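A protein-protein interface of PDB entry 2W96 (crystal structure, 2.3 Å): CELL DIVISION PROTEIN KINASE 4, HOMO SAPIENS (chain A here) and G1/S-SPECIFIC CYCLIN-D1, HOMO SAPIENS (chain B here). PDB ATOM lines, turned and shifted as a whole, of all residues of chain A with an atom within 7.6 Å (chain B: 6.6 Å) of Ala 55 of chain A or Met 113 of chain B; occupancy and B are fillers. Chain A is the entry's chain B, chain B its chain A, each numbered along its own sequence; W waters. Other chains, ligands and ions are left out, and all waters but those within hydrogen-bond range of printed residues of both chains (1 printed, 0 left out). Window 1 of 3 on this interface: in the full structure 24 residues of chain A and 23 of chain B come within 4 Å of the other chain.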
ATOM      1  N   ILE A  48      18.833  30.020  -4.871  1.00  0.00           N
ATOM      2  CA  ILE A  48      18.540  28.665  -4.417  1.00  0.00           C
ATOM      3  C   ILE A  48      17.090  28.246  -4.570  1.00  0.00           C
ATOM      4  O   ILE A  48      16.805  27.099  -4.872  1.00  0.00           O
ATOM      5  CB  ILE A  48      19.025  28.419  -2.978  1.00  0.00           C
ATOM      6  CG1 ILE A  48      20.475  28.861  -2.815  1.00  0.00           C
ATOM      7  CG2 ILE A  48      18.903  26.937  -2.629  1.00  0.00           C
ATOM      8  CD1 ILE A  48      21.176  28.173  -1.649  1.00  0.00           C
ATOM      9  N   SER A  49      16.170  29.153  -4.277  1.00  0.00           N
ATOM     10  CA  SER A  49      14.750  28.821  -4.321  1.00  0.00           C
ATOM     11  C   SER A  49      14.301  28.518  -5.741  1.00  0.00           C
ATOM     12  O   SER A  49      13.452  27.653  -5.969  1.00  0.00           O
ATOM     13  CB  SER A  49      13.914  29.960  -3.729  1.00  0.00           C
ATOM     14  OG  SER A  49      14.219  30.138  -2.355  1.00  0.00           O
ATOM     15  N   THR A  50      14.885  29.231  -6.691  1.00  0.00           N
ATOM     16  CA  THR A  50      14.682  28.954  -8.109  1.00  0.00           C
ATOM     17  C   THR A  50      15.231  27.567  -8.469  1.00  0.00           C
ATOM     18  O   THR A  50      14.513  26.727  -9.014  1.00  0.00           O
ATOM     19  CB  THR A  50      15.321  30.057  -8.969  1.00  0.00           C
ATOM     20  OG1 THR A  50      14.800  31.324  -8.562  1.00  0.00           O
ATOM     21  CG2 THR A  50      15.024  29.845 -10.444  1.00  0.00           C
ATOM     22  N   VAL A  51      16.482  27.306  -8.096  1.00  0.00           N
ATOM     23  CA  VAL A  51      17.074  25.997  -8.339  1.00  0.00           C
ATOM     24  C   VAL A  51      16.236  24.871  -7.761  1.00  0.00           C
ATOM     25  O   VAL A  51      15.946  23.893  -8.456  1.00  0.00           O
ATOM     26  CB  VAL A  51      18.551  25.912  -7.894  1.00  0.00           C
ATOM     27  CG1 VAL A  51      19.315  27.147  -8.308  1.00  0.00           C
ATOM     28  CG2 VAL A  51      18.653  25.676  -6.406  1.00  0.00           C
ATOM     29  N   ARG A  52      15.814  25.022  -6.508  1.00  0.00           N
ATOM     30  CA  ARG A  52      15.038  23.982  -5.829  1.00  0.00           C
ATOM     31  C   ARG A  52      13.622  23.821  -6.395  1.00  0.00           C
ATOM     32  O   ARG A  52      13.176  22.713  -6.670  1.00  0.00           O
ATOM     33  CB  ARG A  52      15.019  24.210  -4.304  1.00  0.00           C
ATOM     34  CG  ARG A  52      16.433  24.300  -3.687  1.00  0.00           C
ATOM     35  CD  ARG A  52      16.486  23.960  -2.185  1.00  0.00           C
ATOM     36  NE  ARG A  52      16.330  25.147  -1.350  1.00  0.00           N
ATOM     37  CZ  ARG A  52      17.244  25.629  -0.508  1.00  0.00           C
ATOM     38  NH1 ARG A  52      18.403  25.011  -0.319  1.00  0.00           N
ATOM     39  NH2 ARG A  52      16.974  26.728   0.181  1.00  0.00           N
ATOM     40  N   GLU A  53      12.947  24.936  -6.642  1.00  0.00           N
ATOM     41  CA  GLU A  53      11.600  24.895  -7.199  1.00  0.00           C
ATOM     42  C   GLU A  53      11.586  24.435  -8.650  1.00  0.00           C
ATOM     43  O   GLU A  53      10.751  23.616  -9.034  1.00  0.00           O
ATOM     44  CB  GLU A  53      10.918  26.259  -7.082  1.00  0.00           C
ATOM     45  CG  GLU A  53      10.671  26.719  -5.663  1.00  0.00           C
ATOM     46  CD  GLU A  53       9.439  26.087  -5.061  1.00  0.00           C
ATOM     47  OE1 GLU A  53       8.349  26.224  -5.661  1.00  0.00           O
ATOM     48  OE2 GLU A  53       9.558  25.468  -3.981  1.00  0.00           O
ATOM     49  N   VAL A  54      12.480  24.978  -9.472  1.00  0.00           N
ATOM     50  CA  VAL A  54      12.571  24.508 -10.860  1.00  0.00           C
ATOM     51  C   VAL A  54      12.913  23.017 -10.933  1.00  0.00           C
ATOM     52  O   VAL A  54      12.343  22.283 -11.746  1.00  0.00           O
ATOM     53  CB  VAL A  54      13.541  25.322 -11.704  1.00  0.00           C
ATOM     54  CG1 VAL A  54      13.865  24.562 -12.968  1.00  0.00           C
ATOM     55  CG2 VAL A  54      12.955  26.683 -12.032  1.00  0.00           C
ATOM     56  N   ALA A  55      13.817  22.574 -10.059  1.00  0.00           N
ATOM     57  CA  ALA A  55      14.225  21.175 -10.012  1.00  0.00           C
ATOM     58  C   ALA A  55      13.077  20.269  -9.611  1.00  0.00           C
ATOM     59  O   ALA A  55      12.976  19.132 -10.074  1.00  0.00           O
ATOM     60  CB  ALA A  55      15.401  20.989  -9.052  1.00  0.00           C
ATOM     61  N   LEU A  56      12.255  20.742  -8.685  1.00  0.00           N
ATOM     62  CA  LEU A  56      11.109  19.964  -8.228  1.00  0.00           C
ATOM     63  C   LEU A  56      10.058  19.793  -9.322  1.00  0.00           C
ATOM     64  O   LEU A  56       9.351  18.791  -9.345  1.00  0.00           O
ATOM     65  CB  LEU A  56      10.484  20.607  -6.984  1.00  0.00           C
ATOM     66  CG  LEU A  56      11.138  20.341  -5.621  1.00  0.00           C
ATOM     67  CD1 LEU A  56      12.664  20.090  -5.699  1.00  0.00           C
ATOM     68  CD2 LEU A  56      10.840  21.526  -4.713  1.00  0.00           C
ATOM     69  N   LEU A  57       9.927  20.787 -10.197  1.00  0.00           N
ATOM     70  CA  LEU A  57       9.029  20.688 -11.352  1.00  0.00           C
ATOM     71  C   LEU A  57       9.591  19.763 -12.421  1.00  0.00           C
ATOM     72  O   LEU A  57       8.853  18.985 -13.024  1.00  0.00           O
ATOM     73  CB  LEU A  57       8.766  22.065 -11.968  1.00  0.00           C
ATOM     74  CG  LEU A  57       8.152  23.120 -11.051  1.00  0.00           C
ATOM     75  CD1 LEU A  57       8.064  24.461 -11.772  1.00  0.00           C
ATOM     76  CD2 LEU A  57       6.793  22.660 -10.553  1.00  0.00           C
ATOM     77  N   ARG A  58      10.894  19.864 -12.675  1.00  0.00           N
ATOM     78  CA  ARG A  58      11.551  18.963 -13.623  1.00  0.00           C
ATOM     79  C   ARG A  58      11.342  17.499 -13.262  1.00  0.00           C
ATOM     80  O   ARG A  58      11.197  16.648 -14.142  1.00  0.00           O
ATOM     81  CB  ARG A  58      13.044  19.275 -13.741  1.00  0.00           C
ATOM     82  CG  ARG A  58      13.344  20.466 -14.630  1.00  0.00           C
ATOM     83  CD  ARG A  58      12.994  20.180 -16.091  1.00  0.00           C
ATOM     84  NE  ARG A  58      14.047  19.426 -16.769  1.00  0.00           N
ATOM     85  CZ  ARG A  58      13.907  18.193 -17.239  1.00  0.00           C
ATOM     86  NH1 ARG A  58      12.744  17.572 -17.139  1.00  0.00           N
ATOM     87  NH2 ARG A  58      14.927  17.591 -17.830  1.00  0.00           N
ATOM     88  N   ARG A  59      11.304  17.211 -11.966  1.00  0.00           N
ATOM     89  CA  ARG A  59      11.206  15.837 -11.500  1.00  0.00           C
ATOM     90  C   ARG A  59       9.812  15.238 -11.664  1.00  0.00           C
ATOM     91  O   ARG A  59       9.672  14.021 -11.762  1.00  0.00           O
ATOM     92  CB  ARG A  59      11.650  15.726 -10.044  1.00  0.00           C
ATOM     93  CG  ARG A  59      11.618  14.288  -9.525  1.00  0.00           C
ATOM     94  CD  ARG A  59      11.265  14.249  -8.047  1.00  0.00           C
ATOM     95  NE  ARG A  59      12.428  14.369  -7.182  1.00  0.00           N
ATOM     96  CZ  ARG A  59      12.389  14.853  -5.945  1.00  0.00           C
ATOM     97  NH1 ARG A  59      11.243  15.301  -5.447  1.00  0.00           N
ATOM     98  NH2 ARG A  59      13.499  14.912  -5.216  1.00  0.00           N
ATOM     99  N   LEU A  60       8.785  16.087 -11.624  1.00  0.00           N
ATOM    100  CA  LEU A  60       7.401  15.653 -11.836  1.00  0.00           C
ATOM    101  C   LEU A  60       7.237  14.802 -13.088  1.00  0.00           C
ATOM    102  O   LEU A  60       6.546  13.785 -13.068  1.00  0.00           O
ATOM    103  CB  LEU A  60       6.467  16.859 -11.939  1.00  0.00           C
ATOM    104  CG  LEU A  60       6.026  17.546 -10.650  1.00  0.00           C
ATOM    105  CD1 LEU A  60       4.982  18.605 -10.966  1.00  0.00           C
ATOM    106  CD2 LEU A  60       5.481  16.535  -9.654  1.00  0.00           C
ATOM    107  N   LEU A  71       7.166  19.933 -17.568  1.00  0.00           N
ATOM    108  CA  LEU A  71       8.290  20.831 -17.809  1.00  0.00           C
ATOM    109  C   LEU A  71       9.411  19.953 -18.323  1.00  0.00           C
ATOM    110  O   LEU A  71       9.868  19.047 -17.621  1.00  0.00           O
ATOM    111  CB  LEU A  71       8.736  21.521 -16.517  1.00  0.00           C
ATOM    112  CG  LEU A  71       9.980  22.407 -16.668  1.00  0.00           C
ATOM    113  CD1 LEU A  71       9.723  23.565 -17.615  1.00  0.00           C
ATOM    114  CD2 LEU A  71      10.455  22.908 -15.320  1.00  0.00           C
ATOM    115  N   VAL A  74      14.964  23.357 -19.269  1.00  0.00           N
ATOM    116  CA  VAL A  74      15.244  24.652 -18.677  1.00  0.00           C
ATOM    117  C   VAL A  74      16.612  25.136 -19.131  1.00  0.00           C
ATOM    118  O   VAL A  74      17.552  24.353 -19.246  1.00  0.00           O
ATOM    119  CB  VAL A  74      15.145  24.612 -17.144  1.00  0.00           C
ATOM    120  CG1 VAL A  74      15.436  25.993 -16.558  1.00  0.00           C
ATOM    121  CG2 VAL A  74      13.769  24.104 -16.718  1.00  0.00           C
ATOM    122  N   ILE A 161       8.937  31.030  -8.191  1.00  0.00           N
ATOM    123  CA  ILE A 161       9.903  31.255  -9.258  1.00  0.00           C
ATOM    124  C   ILE A 161       9.742  32.659  -9.835  1.00  0.00           C
ATOM    125  O   ILE A 161      10.724  33.341 -10.137  1.00  0.00           O
ATOM    126  CB  ILE A 161       9.761  30.189 -10.354  1.00  0.00           C
ATOM    127  CG1 ILE A 161      10.363  28.862  -9.887  1.00  0.00           C
ATOM    128  CG2 ILE A 161      10.397  30.674 -11.658  1.00  0.00           C
ATOM    129  CD1 ILE A 161       9.893  27.667 -10.688  1.00  0.00           C
ATOM    130  N   LEU B  80      24.895  12.930  -4.293  1.00  0.00           N
ATOM    131  CA  LEU B  80      24.211  13.786  -5.259  1.00  0.00           C
ATOM    132  C   LEU B  80      25.197  14.529  -6.158  1.00  0.00           C
ATOM    133  O   LEU B  80      25.018  14.608  -7.372  1.00  0.00           O
ATOM    134  CB  LEU B  80      23.301  14.787  -4.541  1.00  0.00           C
ATOM    135  CG  LEU B  80      22.451  15.723  -5.409  1.00  0.00           C
ATOM    136  CD1 LEU B  80      21.508  14.962  -6.347  1.00  0.00           C
ATOM    137  CD2 LEU B  80      21.669  16.691  -4.534  1.00  0.00           C
ATOM    138  N   TYR B  84      25.832  14.241 -10.314  1.00  0.00           N
ATOM    139  CA  TYR B  84      26.028  15.412 -11.149  1.00  0.00           C
ATOM    140  C   TYR B  84      27.285  15.248 -12.001  1.00  0.00           C
ATOM    141  O   TYR B  84      27.276  15.510 -13.212  1.00  0.00           O
ATOM    142  CB  TYR B  84      26.166  16.656 -10.265  1.00  0.00           C
ATOM    143  CG  TYR B  84      24.877  17.119  -9.610  1.00  0.00           C
ATOM    144  CD1 TYR B  84      23.650  16.567  -9.958  1.00  0.00           C
ATOM    145  CD2 TYR B  84      24.888  18.114  -8.647  1.00  0.00           C
ATOM    146  CE1 TYR B  84      22.478  16.997  -9.364  1.00  0.00           C
ATOM    147  CE2 TYR B  84      23.714  18.516  -8.016  1.00  0.00           C
ATOM    148  CZ  TYR B  84      22.516  17.960  -8.389  1.00  0.00           C
ATOM    149  OH  TYR B  84      21.348  18.399  -7.797  1.00  0.00           O
ATOM    150  N   PHE B 108      28.653  22.298  -4.962  1.00  0.00           N
ATOM    151  CA  PHE B 108      27.986  23.584  -4.788  1.00  0.00           C
ATOM    152  C   PHE B 108      26.488  23.483  -5.104  1.00  0.00           C
ATOM    153  O   PHE B 108      25.646  23.852  -4.287  1.00  0.00           O
ATOM    154  CB  PHE B 108      28.660  24.603  -5.709  1.00  0.00           C
ATOM    155  CG  PHE B 108      28.188  26.014  -5.520  1.00  0.00           C
ATOM    156  CD1 PHE B 108      28.433  26.694  -4.327  1.00  0.00           C
ATOM    157  CD2 PHE B 108      27.552  26.685  -6.556  1.00  0.00           C
ATOM    158  CE1 PHE B 108      28.027  28.016  -4.170  1.00  0.00           C
ATOM    159  CE2 PHE B 108      27.158  28.004  -6.406  1.00  0.00           C
ATOM    160  CZ  PHE B 108      27.385  28.668  -5.206  1.00  0.00           C
ATOM    161  N   VAL B 109      26.162  22.924  -6.266  1.00  0.00           N
ATOM    162  CA  VAL B 109      24.774  22.658  -6.634  1.00  0.00           C
ATOM    163  C   VAL B 109      24.091  21.619  -5.733  1.00  0.00           C
ATOM    164  O   VAL B 109      22.957  21.804  -5.313  1.00  0.00           O
ATOM    165  CB  VAL B 109      24.644  22.307  -8.134  1.00  0.00           C
ATOM    166  CG1 VAL B 109      23.192  22.246  -8.532  1.00  0.00           C
ATOM    167  CG2 VAL B 109      25.368  23.334  -8.979  1.00  0.00           C
ATOM    168  N   ALA B 110      24.794  20.537  -5.416  1.00  0.00           N
ATOM    169  CA  ALA B 110      24.261  19.512  -4.521  1.00  0.00           C
ATOM    170  C   ALA B 110      23.975  20.059  -3.127  1.00  0.00           C
ATOM    171  O   ALA B 110      23.019  19.651  -2.470  1.00  0.00           O
ATOM    172  CB  ALA B 110      25.217  18.332  -4.443  1.00  0.00           C
ATOM    173  N   SER B 111      24.832  20.948  -2.648  1.00  0.00           N
ATOM    174  CA  SER B 111      24.599  21.586  -1.353  1.00  0.00           C
ATOM    175  C   SER B 111      23.389  22.519  -1.372  1.00  0.00           C
ATOM    176  O   SER B 111      22.590  22.541  -0.434  1.00  0.00           O
ATOM    177  CB  SER B 111      25.840  22.340  -0.888  1.00  0.00           C
ATOM    178  OG  SER B 111      25.634  22.834   0.415  1.00  0.00           O
ATOM    179  N   LYS B 112      23.245  23.284  -2.445  1.00  0.00           N
ATOM    180  CA  LYS B 112      22.098  24.172  -2.564  1.00  0.00           C
ATOM    181  C   LYS B 112      20.808  23.389  -2.500  1.00  0.00           C
ATOM    182  O   LYS B 112      19.838  23.832  -1.893  1.00  0.00           O
ATOM    183  CB  LYS B 112      22.144  24.960  -3.869  1.00  0.00           C
ATOM    184  CG  LYS B 112      23.195  26.040  -3.929  1.00  0.00           C
ATOM    185  CD  LYS B 112      23.021  26.801  -5.227  1.00  0.00           C
ATOM    186  CE  LYS B 112      23.979  27.954  -5.341  1.00  0.00           C
ATOM    187  NZ  LYS B 112      23.434  28.936  -6.297  1.00  0.00           N
ATOM    188  N   MET B 113      20.821  22.202  -3.106  1.00  0.00           N
ATOM    189  CA  MET B 113      19.647  21.334  -3.175  1.00  0.00           C
ATOM    190  C   MET B 113      19.293  20.672  -1.852  1.00  0.00           C
ATOM    191  O   MET B 113      18.127  20.433  -1.566  1.00  0.00           O
ATOM    192  CB  MET B 113      19.865  20.245  -4.229  1.00  0.00           C
ATOM    193  CG  MET B 113      19.861  20.759  -5.646  1.00  0.00           C
ATOM    194  SD  MET B 113      18.240  21.372  -6.150  1.00  0.00           S
ATOM    195  CE  MET B 113      17.249  19.949  -5.938  1.00  0.00           C
ATOM    196  N   LYS B 114      20.302  20.313  -1.072  1.00  0.00           N
ATOM    197  CA  LYS B 114      20.080  19.451   0.081  1.00  0.00           C
ATOM    198  C   LYS B 114      20.336  20.079   1.460  1.00  0.00           C
ATOM    199  O   LYS B 114      20.058  19.450   2.479  1.00  0.00           O
ATOM    200  CB  LYS B 114      20.898  18.169  -0.071  1.00  0.00           C
ATOM    201  CG  LYS B 114      20.449  17.288  -1.230  1.00  0.00           C
ATOM    202  CD  LYS B 114      19.186  16.526  -0.869  1.00  0.00           C
ATOM    203  CE  LYS B 114      18.513  15.968  -2.101  1.00  0.00           C
ATOM    204  NZ  LYS B 114      17.329  15.139  -1.747  1.00  0.00           N
ATOM    205  N   GLU B 115      20.899  21.286   1.510  1.00  0.00           N
ATOM    206  CA  GLU B 115      21.273  21.855   2.809  1.00  0.00           C
ATOM    207  C   GLU B 115      20.488  23.097   3.213  1.00  0.00           C
ATOM    208  O   GLU B 115      20.108  23.918   2.368  1.00  0.00           O
ATOM    209  CB  GLU B 115      22.779  22.108   2.894  1.00  0.00           C
ATOM    210  CG  GLU B 115      23.603  20.969   2.332  1.00  0.00           C
ATOM    211  CD  GLU B 115      24.972  20.861   2.952  1.00  0.00           C
ATOM    212  OE1 GLU B 115      25.936  21.401   2.370  1.00  0.00           O
ATOM    213  OE2 GLU B 115      25.092  20.205   4.004  1.00  0.00           O
ATOM    214  N   PRO B 118      23.724  26.066   2.661  1.00  0.00           N
ATOM    215  CA  PRO B 118      24.609  25.487   1.635  1.00  0.00           C
ATOM    216  C   PRO B 118      26.043  25.987   1.746  1.00  0.00           C
ATOM    217  O   PRO B 118      26.289  27.052   2.306  1.00  0.00           O
ATOM    218  CB  PRO B 118      23.998  25.981   0.312  1.00  0.00           C
ATOM    219  CG  PRO B 118      22.701  26.656   0.670  1.00  0.00           C
ATOM    220  CD  PRO B 118      22.831  27.090   2.093  1.00  0.00           C
ATOM    221  N   TRP B 150      18.547  21.217 -15.592  1.00  0.00           N
ATOM    222  CA  TRP B 150      17.974  21.579 -14.287  1.00  0.00           C
ATOM    223  C   TRP B 150      17.249  20.428 -13.589  1.00  0.00           C
ATOM    224  O   TRP B 150      16.543  20.639 -12.603  1.00  0.00           O
ATOM    225  CB  TRP B 150      17.057  22.797 -14.387  1.00  0.00           C
ATOM    226  CG  TRP B 150      17.768  24.101 -14.717  1.00  0.00           C
ATOM    227  CD1 TRP B 150      18.436  24.404 -15.872  1.00  0.00           C
ATOM    228  CD2 TRP B 150      17.784  25.295 -13.922  1.00  0.00           C
ATOM    229  NE1 TRP B 150      18.896  25.697 -15.829  1.00  0.00           N
ATOM    230  CE2 TRP B 150      18.499  26.274 -14.650  1.00  0.00           C
ATOM    231  CE3 TRP B 150      17.242  25.642 -12.672  1.00  0.00           C
ATOM    232  CZ2 TRP B 150      18.698  27.575 -14.172  1.00  0.00           C
ATOM    233  CZ3 TRP B 150      17.461  26.928 -12.183  1.00  0.00           C
ATOM    234  CH2 TRP B 150      18.177  27.881 -12.939  1.00  0.00           C
ATOM    235  N   ASN B 151      17.450  19.208 -14.083  1.00  0.00           N
ATOM    236  CA  ASN B 151      16.925  18.033 -13.401  1.00  0.00           C
ATOM    237  C   ASN B 151      17.872  17.628 -12.263  1.00  0.00           C
ATOM    238  O   ASN B 151      18.568  16.612 -12.340  1.00  0.00           O
ATOM    239  CB  ASN B 151      16.725  16.888 -14.395  1.00  0.00           C
ATOM    240  CG  ASN B 151      15.933  15.732 -13.810  1.00  0.00           C
ATOM    241  OD1 ASN B 151      15.397  15.820 -12.705  1.00  0.00           O
ATOM    242  ND2 ASN B 151      15.877  14.629 -14.544  1.00  0.00           N
ATOM    243  N   LEU B 152      17.887  18.445 -11.210  1.00  0.00           N
ATOM    244  CA  LEU B 152      18.862  18.335 -10.131  1.00  0.00           C
ATOM    245  C   LEU B 152      18.331  17.533  -8.949  1.00  0.00           C
ATOM    246  O   LEU B 152      19.081  17.180  -8.042  1.00  0.00           O
ATOM    247  CB  LEU B 152      19.246  19.732  -9.651  1.00  0.00           C
ATOM    248  CG  LEU B 152      19.601  20.745 -10.738  1.00  0.00           C
ATOM    249  CD1 LEU B 152      19.861  22.125 -10.151  1.00  0.00           C
ATOM    250  CD2 LEU B 152      20.782  20.273 -11.581  1.00  0.00           C
ATOM    251  N   ALA B 153      17.025  17.288  -8.943  1.00  0.00           N
ATOM    252  CA  ALA B 153      16.370  16.609  -7.829  1.00  0.00           C
ATOM    253  C   ALA B 153      16.494  15.097  -7.978  1.00  0.00           C
ATOM    254  O   ALA B 153      15.499  14.370  -7.989  1.00  0.00           O
ATOM    255  CB  ALA B 153      14.909  17.025  -7.748  1.00  0.00           C
ATOM    256  N   ALA B 154      17.733  14.637  -8.117  1.00  0.00           N
ATOM    257  CA  ALA B 154      18.002  13.230  -8.306  1.00  0.00           C
ATOM    258  C   ALA B 154      17.886  12.478  -6.989  1.00  0.00           C
ATOM    259  O   ALA B 154      18.046  13.059  -5.919  1.00  0.00           O
ATOM    260  CB  ALA B 154      19.368  13.041  -8.916  1.00  0.00           C
HETATM  261  O   HOH W   1      14.932  17.430 -10.609  1.00  0.00           O
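O of Lys 112 of chain B is in hydrogen-bond range of NH1 of Arg 52 of chain A, at 2.4 Å. The guanidinium group of Arg 52 of chain A sits at hydrogen-bond distance from the backbone carbonyl oxygen of Glu 115 of chain B. NE of Arg 59 of chain A lies within hydrogen-bond range of O of Ala 153 of chain B, 3.2 Å away.
Ala 55 of chain A touches just these residues of chain B: Met 113 (3.8 Å), Trp 150 (3.5 Å) and Ala 153 (3.7 Å). Of the printed residues of chain A, Met 113 of chain B touches Arg 52 and Ala 55. Printed residues of chain A within 4 Å of Glu 115 of chain B: Arg 52. Of the printed residues of chain A, Lys 112 of chain B touches Ile 48 and Arg 52. Printed residues of chain B within 4 Å of Val 74 of chain A: Trp 150 (3.5 Å). Of the printed residues of chain A, Ala 153 of chain B touches Ala 55 (3.7 Å) and Arg 59 (3.2 Å). Of the printed residues of chain B, Val 54 of chain A touches Trp 150. Thr 50 of chain A touches none of the printed residues of chain B. Phe 108 of chain B touches none of the printed residues of chain A. The nearest printed residue of chain A that does not touch Glu 115 of chain B is Ile 48 of chain A (5.9 Å).
The backbone carbonyl oxygen (O) of Leu 71 of chain A is in hydrogen-bond range of the guanidinium group (NH1) of Arg 58 of chain A, 3.3 Å away. OE1 of Glu 115 of chain B lies within hydrogen-bond range of OG of Ser 111 of chain B (2.4 Å).
Among the printed residues, pairs that only touch across the chains: Ile 48 of chain A with Lys 112 of chain B (3.3 Å), Ile 48 of chain A with Pro 118 of chain B (3.2 Å), Val 51 of chain A with Trp 150 of chain B (3.97 Å), Arg 52 of chain A with Met 113 of chain B (3.9 Å), Val 54 of chain A with Trp 150 of chain B (3.6 Å), Ala 55 of chain A with Met 113 of chain B (3.8 Å), Ala 55 of chain A with Trp 150 of chain B (3.5 Å), Ala 55 of chain A with Ala 153 of chain B (3.7 Å), Arg 58 of chain A with Trp 150 of chain B (3.8 Å), Arg 58 of chain A with Asn 151 of chain B (3.9 Å) and Val 74 of chain A with Trp 150 of chain B (3.5 Å).
Water W1 lies within hydrogen-bond range of O of Ala 55 of chain A (2.6 Å), N of Ala 153 of chain B (2.7 Å), OD1 of Asn 151 of chain B (2.7 Å) and N of Leu 152 of chain B (3.2 Å).
Hydrophobic or aromatic side chains of chain A within 4 Å of the printed part of chain B: Ile 48, Val 54, Ala 55 and Val 74. Printed residues of chain B that touch a printed residue of chain A: Lys 112, Met 113, Glu 115, Pro 118, Trp 150, Asn 151 and Ala 153. Hydrophobic or aromatic side chains of chain B that line the printed part of chain A: Met 113, Pro 118, Trp 150 and Ala 153. Among the printed residues, no Asp or Glu carboxylate lies within 4 Å of a Lys or Arg side-chain nitrogen of the other chain.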
